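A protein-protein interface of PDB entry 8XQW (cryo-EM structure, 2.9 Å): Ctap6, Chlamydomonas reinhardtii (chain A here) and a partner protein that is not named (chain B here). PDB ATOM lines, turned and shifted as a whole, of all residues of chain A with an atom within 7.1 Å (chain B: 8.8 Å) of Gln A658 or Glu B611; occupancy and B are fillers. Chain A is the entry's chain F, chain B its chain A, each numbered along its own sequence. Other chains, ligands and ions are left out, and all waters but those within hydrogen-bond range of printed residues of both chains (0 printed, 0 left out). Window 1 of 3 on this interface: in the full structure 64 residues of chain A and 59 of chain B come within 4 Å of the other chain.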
ATOM      1  N   ARG A 655      29.987   3.523 -23.190  1.00  0.00           N
ATOM      2  CA  ARG A 655      30.306   4.690 -22.388  1.00  0.00           C
ATOM      3  C   ARG A 655      29.591   4.618 -21.040  1.00  0.00           C
ATOM      4  O   ARG A 655      28.771   3.731 -20.786  1.00  0.00           O
ATOM      5  CB  ARG A 655      29.935   5.968 -23.137  1.00  0.00           C
ATOM      6  CG  ARG A 655      31.141   6.715 -23.668  1.00  0.00           C
ATOM      7  CD  ARG A 655      30.832   7.436 -24.965  1.00  0.00           C
ATOM      8  NE  ARG A 655      32.046   7.734 -25.721  1.00  0.00           N
ATOM      9  CZ  ARG A 655      32.933   8.667 -25.386  1.00  0.00           C
ATOM     10  NH1 ARG A 655      34.007   8.861 -26.137  1.00  0.00           N
ATOM     11  NH2 ARG A 655      32.738   9.417 -24.310  1.00  0.00           N
ATOM     12  N   GLN A 656      29.915   5.572 -20.173  1.00  0.00           N
ATOM     13  CA  GLN A 656      29.392   5.562 -18.814  1.00  0.00           C
ATOM     14  C   GLN A 656      27.871   5.632 -18.813  1.00  0.00           C
ATOM     15  O   GLN A 656      27.269   6.469 -19.489  1.00  0.00           O
ATOM     16  CB  GLN A 656      29.966   6.732 -18.018  1.00  0.00           C
ATOM     17  CG  GLN A 656      29.681   6.665 -16.528  1.00  0.00           C
ATOM     18  CD  GLN A 656      29.929   5.290 -15.941  1.00  0.00           C
ATOM     19  OE1 GLN A 656      31.068   4.826 -15.875  1.00  0.00           O
ATOM     20  NE2 GLN A 656      28.862   4.631 -15.506  1.00  0.00           N
ATOM     21  N   ARG A 657      27.249   4.740 -18.047  1.00  0.00           N
ATOM     22  CA  ARG A 657      25.803   4.771 -17.894  1.00  0.00           C
ATOM     23  C   ARG A 657      25.391   5.933 -17.003  1.00  0.00           C
ATOM     24  O   ARG A 657      25.690   5.954 -15.806  1.00  0.00           O
ATOM     25  CB  ARG A 657      25.301   3.462 -17.288  1.00  0.00           C
ATOM     26  CG  ARG A 657      25.767   2.207 -17.998  1.00  0.00           C
ATOM     27  CD  ARG A 657      24.879   1.030 -17.633  1.00  0.00           C
ATOM     28  NE  ARG A 657      25.564   0.087 -16.757  1.00  0.00           N
ATOM     29  CZ  ARG A 657      24.942  -0.800 -15.987  1.00  0.00           C
ATOM     30  NH1 ARG A 657      23.619  -0.860 -15.981  1.00  0.00           N
ATOM     31  NH2 ARG A 657      25.643  -1.619 -15.218  1.00  0.00           N
ATOM     32  N   GLN A 658      24.682   6.893 -17.589  1.00  0.00           N
ATOM     33  CA  GLN A 658      24.170   8.043 -16.860  1.00  0.00           C
ATOM     34  C   GLN A 658      23.035   8.653 -17.670  1.00  0.00           C
ATOM     35  O   GLN A 658      22.660   8.147 -18.731  1.00  0.00           O
ATOM     36  CB  GLN A 658      25.263   9.084 -16.579  1.00  0.00           C
ATOM     37  CG  GLN A 658      26.032   8.910 -15.259  1.00  0.00           C
ATOM     38  CD  GLN A 658      25.134   8.614 -14.060  1.00  0.00           C
ATOM     39  OE1 GLN A 658      24.768   9.518 -13.309  1.00  0.00           O
ATOM     40  NE2 GLN A 658      24.809   7.340 -13.858  1.00  0.00           N
ATOM     41  N   GLY A 659      22.487   9.752 -17.154  1.00  0.00           N
ATOM     42  CA  GLY A 659      21.337  10.380 -17.773  1.00  0.00           C
ATOM     43  C   GLY A 659      21.615  10.927 -19.157  1.00  0.00           C
ATOM     44  O   GLY A 659      21.119  10.389 -20.149  1.00  0.00           O
ATOM     45  N   GLY A 660      22.419  11.988 -19.231  1.00  0.00           N
ATOM     46  CA  GLY A 660      22.801  12.548 -20.520  1.00  0.00           C
ATOM     47  C   GLY A 660      21.596  12.873 -21.382  1.00  0.00           C
ATOM     48  O   GLY A 660      20.739  13.684 -21.017  1.00  0.00           O
ATOM     49  N   GLY A 661      21.532  12.236 -22.551  1.00  0.00           N
ATOM     50  CA  GLY A 661      20.430  12.410 -23.468  1.00  0.00           C
ATOM     51  C   GLY A 661      19.323  11.398 -23.245  1.00  0.00           C
ATOM     52  O   GLY A 661      19.330  10.616 -22.293  1.00  0.00           O
ATOM     53  N   ASN A 664      20.032   7.331 -23.909  1.00  0.00           N
ATOM     54  CA  ASN A 664      20.572   6.452 -22.883  1.00  0.00           C
ATOM     55  C   ASN A 664      19.518   5.524 -22.304  1.00  0.00           C
ATOM     56  O   ASN A 664      19.873   4.474 -21.764  1.00  0.00           O
ATOM     57  CB  ASN A 664      21.225   7.274 -21.771  1.00  0.00           C
ATOM     58  CG  ASN A 664      22.385   8.122 -22.269  1.00  0.00           C
ATOM     59  OD1 ASN A 664      22.987   8.875 -21.506  1.00  0.00           O
ATOM     60  ND2 ASN A 664      22.712   7.994 -23.551  1.00  0.00           N
ATOM     61  N   ASP A 665      18.232   5.875 -22.407  1.00  0.00           N
ATOM     62  CA  ASP A 665      17.199   4.934 -21.991  1.00  0.00           C
ATOM     63  C   ASP A 665      17.243   3.666 -22.831  1.00  0.00           C
ATOM     64  O   ASP A 665      16.785   2.607 -22.388  1.00  0.00           O
ATOM     65  CB  ASP A 665      15.819   5.587 -22.077  1.00  0.00           C
ATOM     66  CG  ASP A 665      14.837   5.007 -21.079  1.00  0.00           C
ATOM     67  OD1 ASP A 665      15.114   5.070 -19.863  1.00  0.00           O
ATOM     68  OD2 ASP A 665      13.790   4.486 -21.512  1.00  0.00           O
ATOM     69  N   ARG A 667      20.438   3.230 -24.940  1.00  0.00           N
ATOM     70  CA  ARG A 667      21.853   2.973 -25.182  1.00  0.00           C
ATOM     71  C   ARG A 667      22.460   2.084 -24.105  1.00  0.00           C
ATOM     72  O   ARG A 667      23.097   1.071 -24.411  1.00  0.00           O
ATOM     73  CB  ARG A 667      22.615   4.295 -25.274  1.00  0.00           C
ATOM     74  CG  ARG A 667      23.984   4.176 -25.913  1.00  0.00           C
ATOM     75  CD  ARG A 667      25.078   4.079 -24.866  1.00  0.00           C
ATOM     76  NE  ARG A 667      25.316   5.357 -24.205  1.00  0.00           N
ATOM     77  CZ  ARG A 667      26.117   5.515 -23.157  1.00  0.00           C
ATOM     78  NH1 ARG A 667      26.763   4.475 -22.650  1.00  0.00           N
ATOM     79  NH2 ARG A 667      26.276   6.715 -22.616  1.00  0.00           N
ATOM     80  N   ASP A 668      22.284   2.452 -22.837  1.00  0.00           N
ATOM     81  CA  ASP A 668      22.838   1.620 -21.777  1.00  0.00           C
ATOM     82  C   ASP A 668      22.072   0.316 -21.623  1.00  0.00           C
ATOM     83  O   ASP A 668      22.637  -0.672 -21.138  1.00  0.00           O
ATOM     84  CB  ASP A 668      22.874   2.386 -20.451  1.00  0.00           C
ATOM     85  CG  ASP A 668      21.504   2.860 -20.000  1.00  0.00           C
ATOM     86  OD1 ASP A 668      20.505   2.134 -20.186  1.00  0.00           O
ATOM     87  OD2 ASP A 668      21.426   3.981 -19.451  1.00  0.00           O
ATOM     88  N   GLU B 559      20.079  -7.165 -12.674  1.00  0.00           N
ATOM     89  CA  GLU B 559      20.115  -5.885 -13.376  1.00  0.00           C
ATOM     90  C   GLU B 559      18.708  -5.374 -13.676  1.00  0.00           C
ATOM     91  O   GLU B 559      18.310  -5.224 -14.832  1.00  0.00           O
ATOM     92  CB  GLU B 559      20.944  -5.989 -14.660  1.00  0.00           C
ATOM     93  CG  GLU B 559      21.494  -4.678 -15.231  1.00  0.00           C
ATOM     94  CD  GLU B 559      22.112  -3.734 -14.200  1.00  0.00           C
ATOM     95  OE1 GLU B 559      22.533  -4.187 -13.114  1.00  0.00           O
ATOM     96  OE2 GLU B 559      22.197  -2.523 -14.492  1.00  0.00           O
ATOM     97  N   ILE B 560      17.943  -5.109 -12.618  1.00  0.00           N
ATOM     98  CA  ILE B 560      16.626  -4.503 -12.779  1.00  0.00           C
ATOM     99  C   ILE B 560      16.782  -3.025 -13.106  1.00  0.00           C
ATOM    100  O   ILE B 560      15.796  -2.338 -13.392  1.00  0.00           O
ATOM    101  CB  ILE B 560      15.747  -4.694 -11.530  1.00  0.00           C
ATOM    102  CG1 ILE B 560      16.581  -4.583 -10.261  1.00  0.00           C
ATOM    103  CG2 ILE B 560      15.024  -6.016 -11.570  1.00  0.00           C
ATOM    104  CD1 ILE B 560      15.813  -4.932  -9.020  1.00  0.00           C
ATOM    105  N   ASP B 561      18.019  -2.525 -13.062  1.00  0.00           N
ATOM    106  CA  ASP B 561      18.276  -1.129 -13.402  1.00  0.00           C
ATOM    107  C   ASP B 561      17.723  -0.767 -14.769  1.00  0.00           C
ATOM    108  O   ASP B 561      17.268   0.363 -14.974  1.00  0.00           O
ATOM    109  CB  ASP B 561      19.776  -0.850 -13.367  1.00  0.00           C
ATOM    110  CG  ASP B 561      20.368  -1.050 -11.997  1.00  0.00           C
ATOM    111  OD1 ASP B 561      19.714  -0.637 -11.018  1.00  0.00           O
ATOM    112  OD2 ASP B 561      21.467  -1.640 -11.897  1.00  0.00           O
ATOM    113  N   ALA B 562      17.752  -1.702 -15.713  1.00  0.00           N
ATOM    114  CA  ALA B 562      17.224  -1.447 -17.041  1.00  0.00           C
ATOM    115  C   ALA B 562      15.711  -1.557 -17.102  1.00  0.00           C
ATOM    116  O   ALA B 562      15.111  -1.108 -18.086  1.00  0.00           O
ATOM    117  CB  ALA B 562      17.846  -2.411 -18.051  1.00  0.00           C
ATOM    118  N   ILE B 563      15.080  -2.141 -16.085  1.00  0.00           N
ATOM    119  CA  ILE B 563      13.634  -2.241 -16.043  1.00  0.00           C
ATOM    120  C   ILE B 563      13.023  -1.477 -14.870  1.00  0.00           C
ATOM    121  O   ILE B 563      11.932  -0.915 -15.016  1.00  0.00           O
ATOM    122  CB  ILE B 563      13.179  -3.716 -16.038  1.00  0.00           C
ATOM    123  CG1 ILE B 563      11.769  -3.828 -16.613  1.00  0.00           C
ATOM    124  CG2 ILE B 563      13.251  -4.326 -14.644  1.00  0.00           C
ATOM    125  CD1 ILE B 563      11.631  -3.206 -17.982  1.00  0.00           C
ATOM    126  N   GLY B 564      13.687  -1.434 -13.718  1.00  0.00           N
ATOM    127  CA  GLY B 564      13.141  -0.749 -12.566  1.00  0.00           C
ATOM    128  C   GLY B 564      13.664   0.663 -12.432  1.00  0.00           C
ATOM    129  O   GLY B 564      13.765   1.196 -11.325  1.00  0.00           O
ATOM    130  N   ARG B 565      14.002   1.278 -13.559  1.00  0.00           N
ATOM    131  CA  ARG B 565      14.486   2.647 -13.546  1.00  0.00           C
ATOM    132  C   ARG B 565      13.362   3.599 -13.162  1.00  0.00           C
ATOM    133  O   ARG B 565      12.195   3.383 -13.498  1.00  0.00           O
ATOM    134  CB  ARG B 565      15.048   3.025 -14.912  1.00  0.00           C
ATOM    135  CG  ARG B 565      15.636   4.417 -14.976  1.00  0.00           C
ATOM    136  CD  ARG B 565      15.981   4.791 -16.398  1.00  0.00           C
ATOM    137  NE  ARG B 565      16.659   3.696 -17.082  1.00  0.00           N
ATOM    138  CZ  ARG B 565      17.944   3.405 -16.927  1.00  0.00           C
ATOM    139  NH1 ARG B 565      18.696   4.127 -16.109  1.00  0.00           N
ATOM    140  NH2 ARG B 565      18.478   2.390 -17.590  1.00  0.00           N
ATOM    141  N   ALA B 566      13.725   4.658 -12.442  1.00  0.00           N
ATOM    142  CA  ALA B 566      12.748   5.660 -12.045  1.00  0.00           C
ATOM    143  C   ALA B 566      12.137   6.320 -13.273  1.00  0.00           C
ATOM    144  O   ALA B 566      12.844   6.709 -14.206  1.00  0.00           O
ATOM    145  CB  ALA B 566      13.394   6.715 -11.151  1.00  0.00           C
ATOM    146  N   ARG B 567      10.813   6.438 -13.273  1.00  0.00           N
ATOM    147  CA  ARG B 567      10.092   7.052 -14.382  1.00  0.00           C
ATOM    148  C   ARG B 567      10.416   8.538 -14.392  1.00  0.00           C
ATOM    149  O   ARG B 567      10.337   9.212 -13.362  1.00  0.00           O
ATOM    150  CB  ARG B 567       8.594   6.825 -14.248  1.00  0.00           C
ATOM    151  CG  ARG B 567       8.213   5.505 -13.635  1.00  0.00           C
ATOM    152  CD  ARG B 567       6.721   5.454 -13.420  1.00  0.00           C
ATOM    153  NE  ARG B 567       6.332   4.389 -12.508  1.00  0.00           N
ATOM    154  CZ  ARG B 567       5.086   4.192 -12.095  1.00  0.00           C
ATOM    155  NH1 ARG B 567       4.119   4.989 -12.521  1.00  0.00           N
ATOM    156  NH2 ARG B 567       4.807   3.201 -11.263  1.00  0.00           N
ATOM    157  N   SER B 568      10.787   9.053 -15.558  1.00  0.00           N
ATOM    158  CA  SER B 568      11.093  10.467 -15.704  1.00  0.00           C
ATOM    159  C   SER B 568       9.796  11.234 -15.960  1.00  0.00           C
ATOM    160  O   SER B 568       8.702  10.666 -15.978  1.00  0.00           O
ATOM    161  CB  SER B 568      12.112  10.675 -16.819  1.00  0.00           C
ATOM    162  OG  SER B 568      13.032   9.598 -16.881  1.00  0.00           O
ATOM    163  N   LEU B 583       7.117  -1.749 -15.914  1.00  0.00           N
ATOM    164  CA  LEU B 583       7.312  -1.394 -14.513  1.00  0.00           C
ATOM    165  C   LEU B 583       6.003  -1.495 -13.741  1.00  0.00           C
ATOM    166  O   LEU B 583       5.963  -2.027 -12.628  1.00  0.00           O
ATOM    167  CB  LEU B 583       7.902   0.012 -14.417  1.00  0.00           C
ATOM    168  CG  LEU B 583       8.763   0.430 -13.223  1.00  0.00           C
ATOM    169  CD1 LEU B 583       9.158   1.881 -13.385  1.00  0.00           C
ATOM    170  CD2 LEU B 583       8.077   0.230 -11.894  1.00  0.00           C
ATOM    171  N   THR B 606      21.789  -4.991  -8.280  1.00  0.00           N
ATOM    172  CA  THR B 606      22.079  -3.762  -9.000  1.00  0.00           C
ATOM    173  C   THR B 606      23.388  -3.171  -8.508  1.00  0.00           C
ATOM    174  O   THR B 606      23.822  -3.407  -7.379  1.00  0.00           O
ATOM    175  CB  THR B 606      20.969  -2.720  -8.824  1.00  0.00           C
ATOM    176  OG1 THR B 606      20.797  -2.443  -7.430  1.00  0.00           O
ATOM    177  CG2 THR B 606      19.663  -3.224  -9.379  1.00  0.00           C
ATOM    178  N   ASN B 607      24.017  -2.386  -9.380  1.00  0.00           N
ATOM    179  CA  ASN B 607      25.108  -1.506  -8.995  1.00  0.00           C
ATOM    180  C   ASN B 607      24.736  -0.048  -9.223  1.00  0.00           C
ATOM    181  O   ASN B 607      25.591   0.832  -9.072  1.00  0.00           O
ATOM    182  CB  ASN B 607      26.383  -1.854  -9.763  1.00  0.00           C
ATOM    183  CG  ASN B 607      26.105  -2.210 -11.196  1.00  0.00           C
ATOM    184  OD1 ASN B 607      24.986  -2.047 -11.676  1.00  0.00           O
ATOM    185  ND2 ASN B 607      27.117  -2.708 -11.893  1.00  0.00           N
ATOM    186  N   LEU B 608      23.484   0.220  -9.573  1.00  0.00           N
ATOM    187  CA  LEU B 608      22.952   1.546  -9.859  1.00  0.00           C
ATOM    188  C   LEU B 608      21.732   1.810  -8.996  1.00  0.00           C
ATOM    189  O   LEU B 608      20.664   2.179  -9.482  1.00  0.00           O
ATOM    190  CB  LEU B 608      22.585   1.689 -11.330  1.00  0.00           C
ATOM    191  CG  LEU B 608      23.724   1.768 -12.339  1.00  0.00           C
ATOM    192  CD1 LEU B 608      23.238   2.370 -13.647  1.00  0.00           C
ATOM    193  CD2 LEU B 608      24.873   2.573 -11.772  1.00  0.00           C
ATOM    194  N   ALA B 609      21.874   1.591  -7.689  1.00  0.00           N
ATOM    195  CA  ALA B 609      20.716   1.590  -6.804  1.00  0.00           C
ATOM    196  C   ALA B 609      19.967   2.916  -6.797  1.00  0.00           C
ATOM    197  O   ALA B 609      18.769   2.933  -6.501  1.00  0.00           O
ATOM    198  CB  ALA B 609      21.147   1.228  -5.386  1.00  0.00           C
ATOM    199  N   GLN B 610      20.632   4.026  -7.127  1.00  0.00           N
ATOM    200  CA  GLN B 610      19.972   5.324  -7.034  1.00  0.00           C
ATOM    201  C   GLN B 610      19.015   5.568  -8.193  1.00  0.00           C
ATOM    202  O   GLN B 610      18.209   6.501  -8.134  1.00  0.00           O
ATOM    203  CB  GLN B 610      21.010   6.442  -6.970  1.00  0.00           C
ATOM    204  CG  GLN B 610      21.849   6.599  -8.224  1.00  0.00           C
ATOM    205  CD  GLN B 610      23.033   5.653  -8.257  1.00  0.00           C
ATOM    206  OE1 GLN B 610      23.156   4.766  -7.416  1.00  0.00           O
ATOM    207  NE2 GLN B 610      23.907   5.836  -9.233  1.00  0.00           N
ATOM    208  N   GLU B 611      19.087   4.765  -9.248  1.00  0.00           N
ATOM    209  CA  GLU B 611      18.223   4.939 -10.405  1.00  0.00           C
ATOM    210  C   GLU B 611      16.870   4.271 -10.230  1.00  0.00           C
ATOM    211  O   GLU B 611      15.999   4.418 -11.093  1.00  0.00           O
ATOM    212  CB  GLU B 611      18.905   4.406 -11.661  1.00  0.00           C
ATOM    213  CG  GLU B 611      19.886   5.369 -12.280  1.00  0.00           C
ATOM    214  CD  GLU B 611      21.274   5.222 -11.704  1.00  0.00           C
ATOM    215  OE1 GLU B 611      22.235   5.710 -12.332  1.00  0.00           O
ATOM    216  OE2 GLU B 611      21.404   4.620 -10.623  1.00  0.00           O
ATOM    217  N   LEU B 612      16.673   3.545  -9.139  1.00  0.00           N
ATOM    218  CA  LEU B 612      15.428   2.830  -8.925  1.00  0.00           C
ATOM    219  C   LEU B 612      14.301   3.802  -8.601  1.00  0.00           C
ATOM    220  O   LEU B 612      14.495   4.829  -7.949  1.00  0.00           O
ATOM    221  CB  LEU B 612      15.586   1.813  -7.799  1.00  0.00           C
ATOM    222  CG  LEU B 612      16.699   0.787  -7.969  1.00  0.00           C
ATOM    223  CD1 LEU B 612      16.676  -0.195  -6.819  1.00  0.00           C
ATOM    224  CD2 LEU B 612      16.547   0.067  -9.285  1.00  0.00           C
ATOM    225  N   ASP B 613      13.105   3.461  -9.059  1.00  0.00           N
ATOM    226  CA  ASP B 613      11.907   4.223  -8.750  1.00  0.00           C
ATOM    227  C   ASP B 613      11.492   3.937  -7.316  1.00  0.00           C
ATOM    228  O   ASP B 613      11.516   2.785  -6.871  1.00  0.00           O
ATOM    229  CB  ASP B 613      10.770   3.870  -9.710  1.00  0.00           C
ATOM    230  CG  ASP B 613       9.461   4.541  -9.345  1.00  0.00           C
ATOM    231  OD1 ASP B 613       9.493   5.611  -8.702  1.00  0.00           O
ATOM    232  OD2 ASP B 613       8.399   3.997  -9.702  1.00  0.00           O
ATOM    233  N   ALA B 614      11.119   4.990  -6.591  1.00  0.00           N
ATOM    234  CA  ALA B 614      10.742   4.823  -5.196  1.00  0.00           C
ATOM    235  C   ALA B 614       9.456   4.030  -5.026  1.00  0.00           C
ATOM    236  O   ALA B 614       9.150   3.613  -3.904  1.00  0.00           O
ATOM    237  CB  ALA B 614      10.605   6.188  -4.523  1.00  0.00           C
ATOM    238  N   LEU B 616       9.140   1.149  -6.133  1.00  0.00           N
ATOM    239  CA  LEU B 616       9.601  -0.220  -5.937  1.00  0.00           C
ATOM    240  C   LEU B 616      10.000  -0.462  -4.490  1.00  0.00           C
ATOM    241  O   LEU B 616       9.706  -1.520  -3.922  1.00  0.00           O
ATOM    242  CB  LEU B 616      10.768  -0.520  -6.875  1.00  0.00           C
ATOM    243  CG  LEU B 616      10.450  -1.384  -8.094  1.00  0.00           C
ATOM    244  CD1 LEU B 616       9.127  -0.986  -8.698  1.00  0.00           C
ATOM    245  CD2 LEU B 616      11.552  -1.283  -9.128  1.00  0.00           C
ATOM    246  N   LEU B 617      10.676   0.505  -3.876  1.00  0.00           N
ATOM    247  CA  LEU B 617      11.203   0.309  -2.532  1.00  0.00           C
ATOM    248  C   LEU B 617      10.185   0.598  -1.440  1.00  0.00           C
ATOM    249  O   LEU B 617      10.542   0.532  -0.260  1.00  0.00           O
ATOM    250  CB  LEU B 617      12.448   1.169  -2.339  1.00  0.00           C
ATOM    251  CG  LEU B 617      13.622   0.857  -3.268  1.00  0.00           C
ATOM    252  CD1 LEU B 617      14.902   1.126  -2.533  1.00  0.00           C
ATOM    253  CD2 LEU B 617      13.600  -0.581  -3.732  1.00  0.00           C
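Of the 22 printed residues of chain B, 4 touch a printed residue of chain A.
Among the printed residues, Asp or Glu carboxylates within 4 Å of a Lys or Arg side-chain nitrogen of the other chain: Arg A657 with Glu B559 (2.6 Å), Asp A665 with Arg B565 (3.5 Å) and Asp A668 with Arg B565 (3.3 Å).
Of the printed residues of chain A, Arg B565 touches Asp A665 and Asp A668.
Of the printed residues of chain A, Asn B607 touches Arg A657 (3.6 Å).
Of chain A, only Gln A658 comes within 4 Å of Glu B611.
The nearest residue of chain B that does not touch Gln A658 is Gln B610 (4.9 Å).
The nearest printed residue of chain A that does not touch Glu B559 is Asp A668 (6.9 Å).
OE2 of Glu B559 lies within salt-bridge range of NH1 of Arg A657 (2.6 Å).
The side-chain carboxylate (OD1) of Asp A665 is in salt-bridge range of the guanidinium group (NE) of Arg B565 (3.5 Å).
The side-chain carboxylate of Asp A668 is in salt-bridge range of the guanidinium group of Arg B565 (3.3 Å).
The side-chain amide nitrogen of Gln A658 is in hydrogen-bond range of the side-chain carboxylate of Glu B611 (3.4 Å).
Among the printed residues, merely in contact across the chains: Arg A657 with Asn B607.
N of Ala B566 lies within hydrogen-bond range of O of Glu B611 (2.7 Å).
The side-chain amide nitrogen of Gln B610 lies close to the side-chain carboxylate of Glu B611 (3.1 Å).
The backbone carbonyl oxygen (O) of Gln A658 lies close to the side-chain amide oxygen (OD1) of Asn A664 (2.9 Å).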
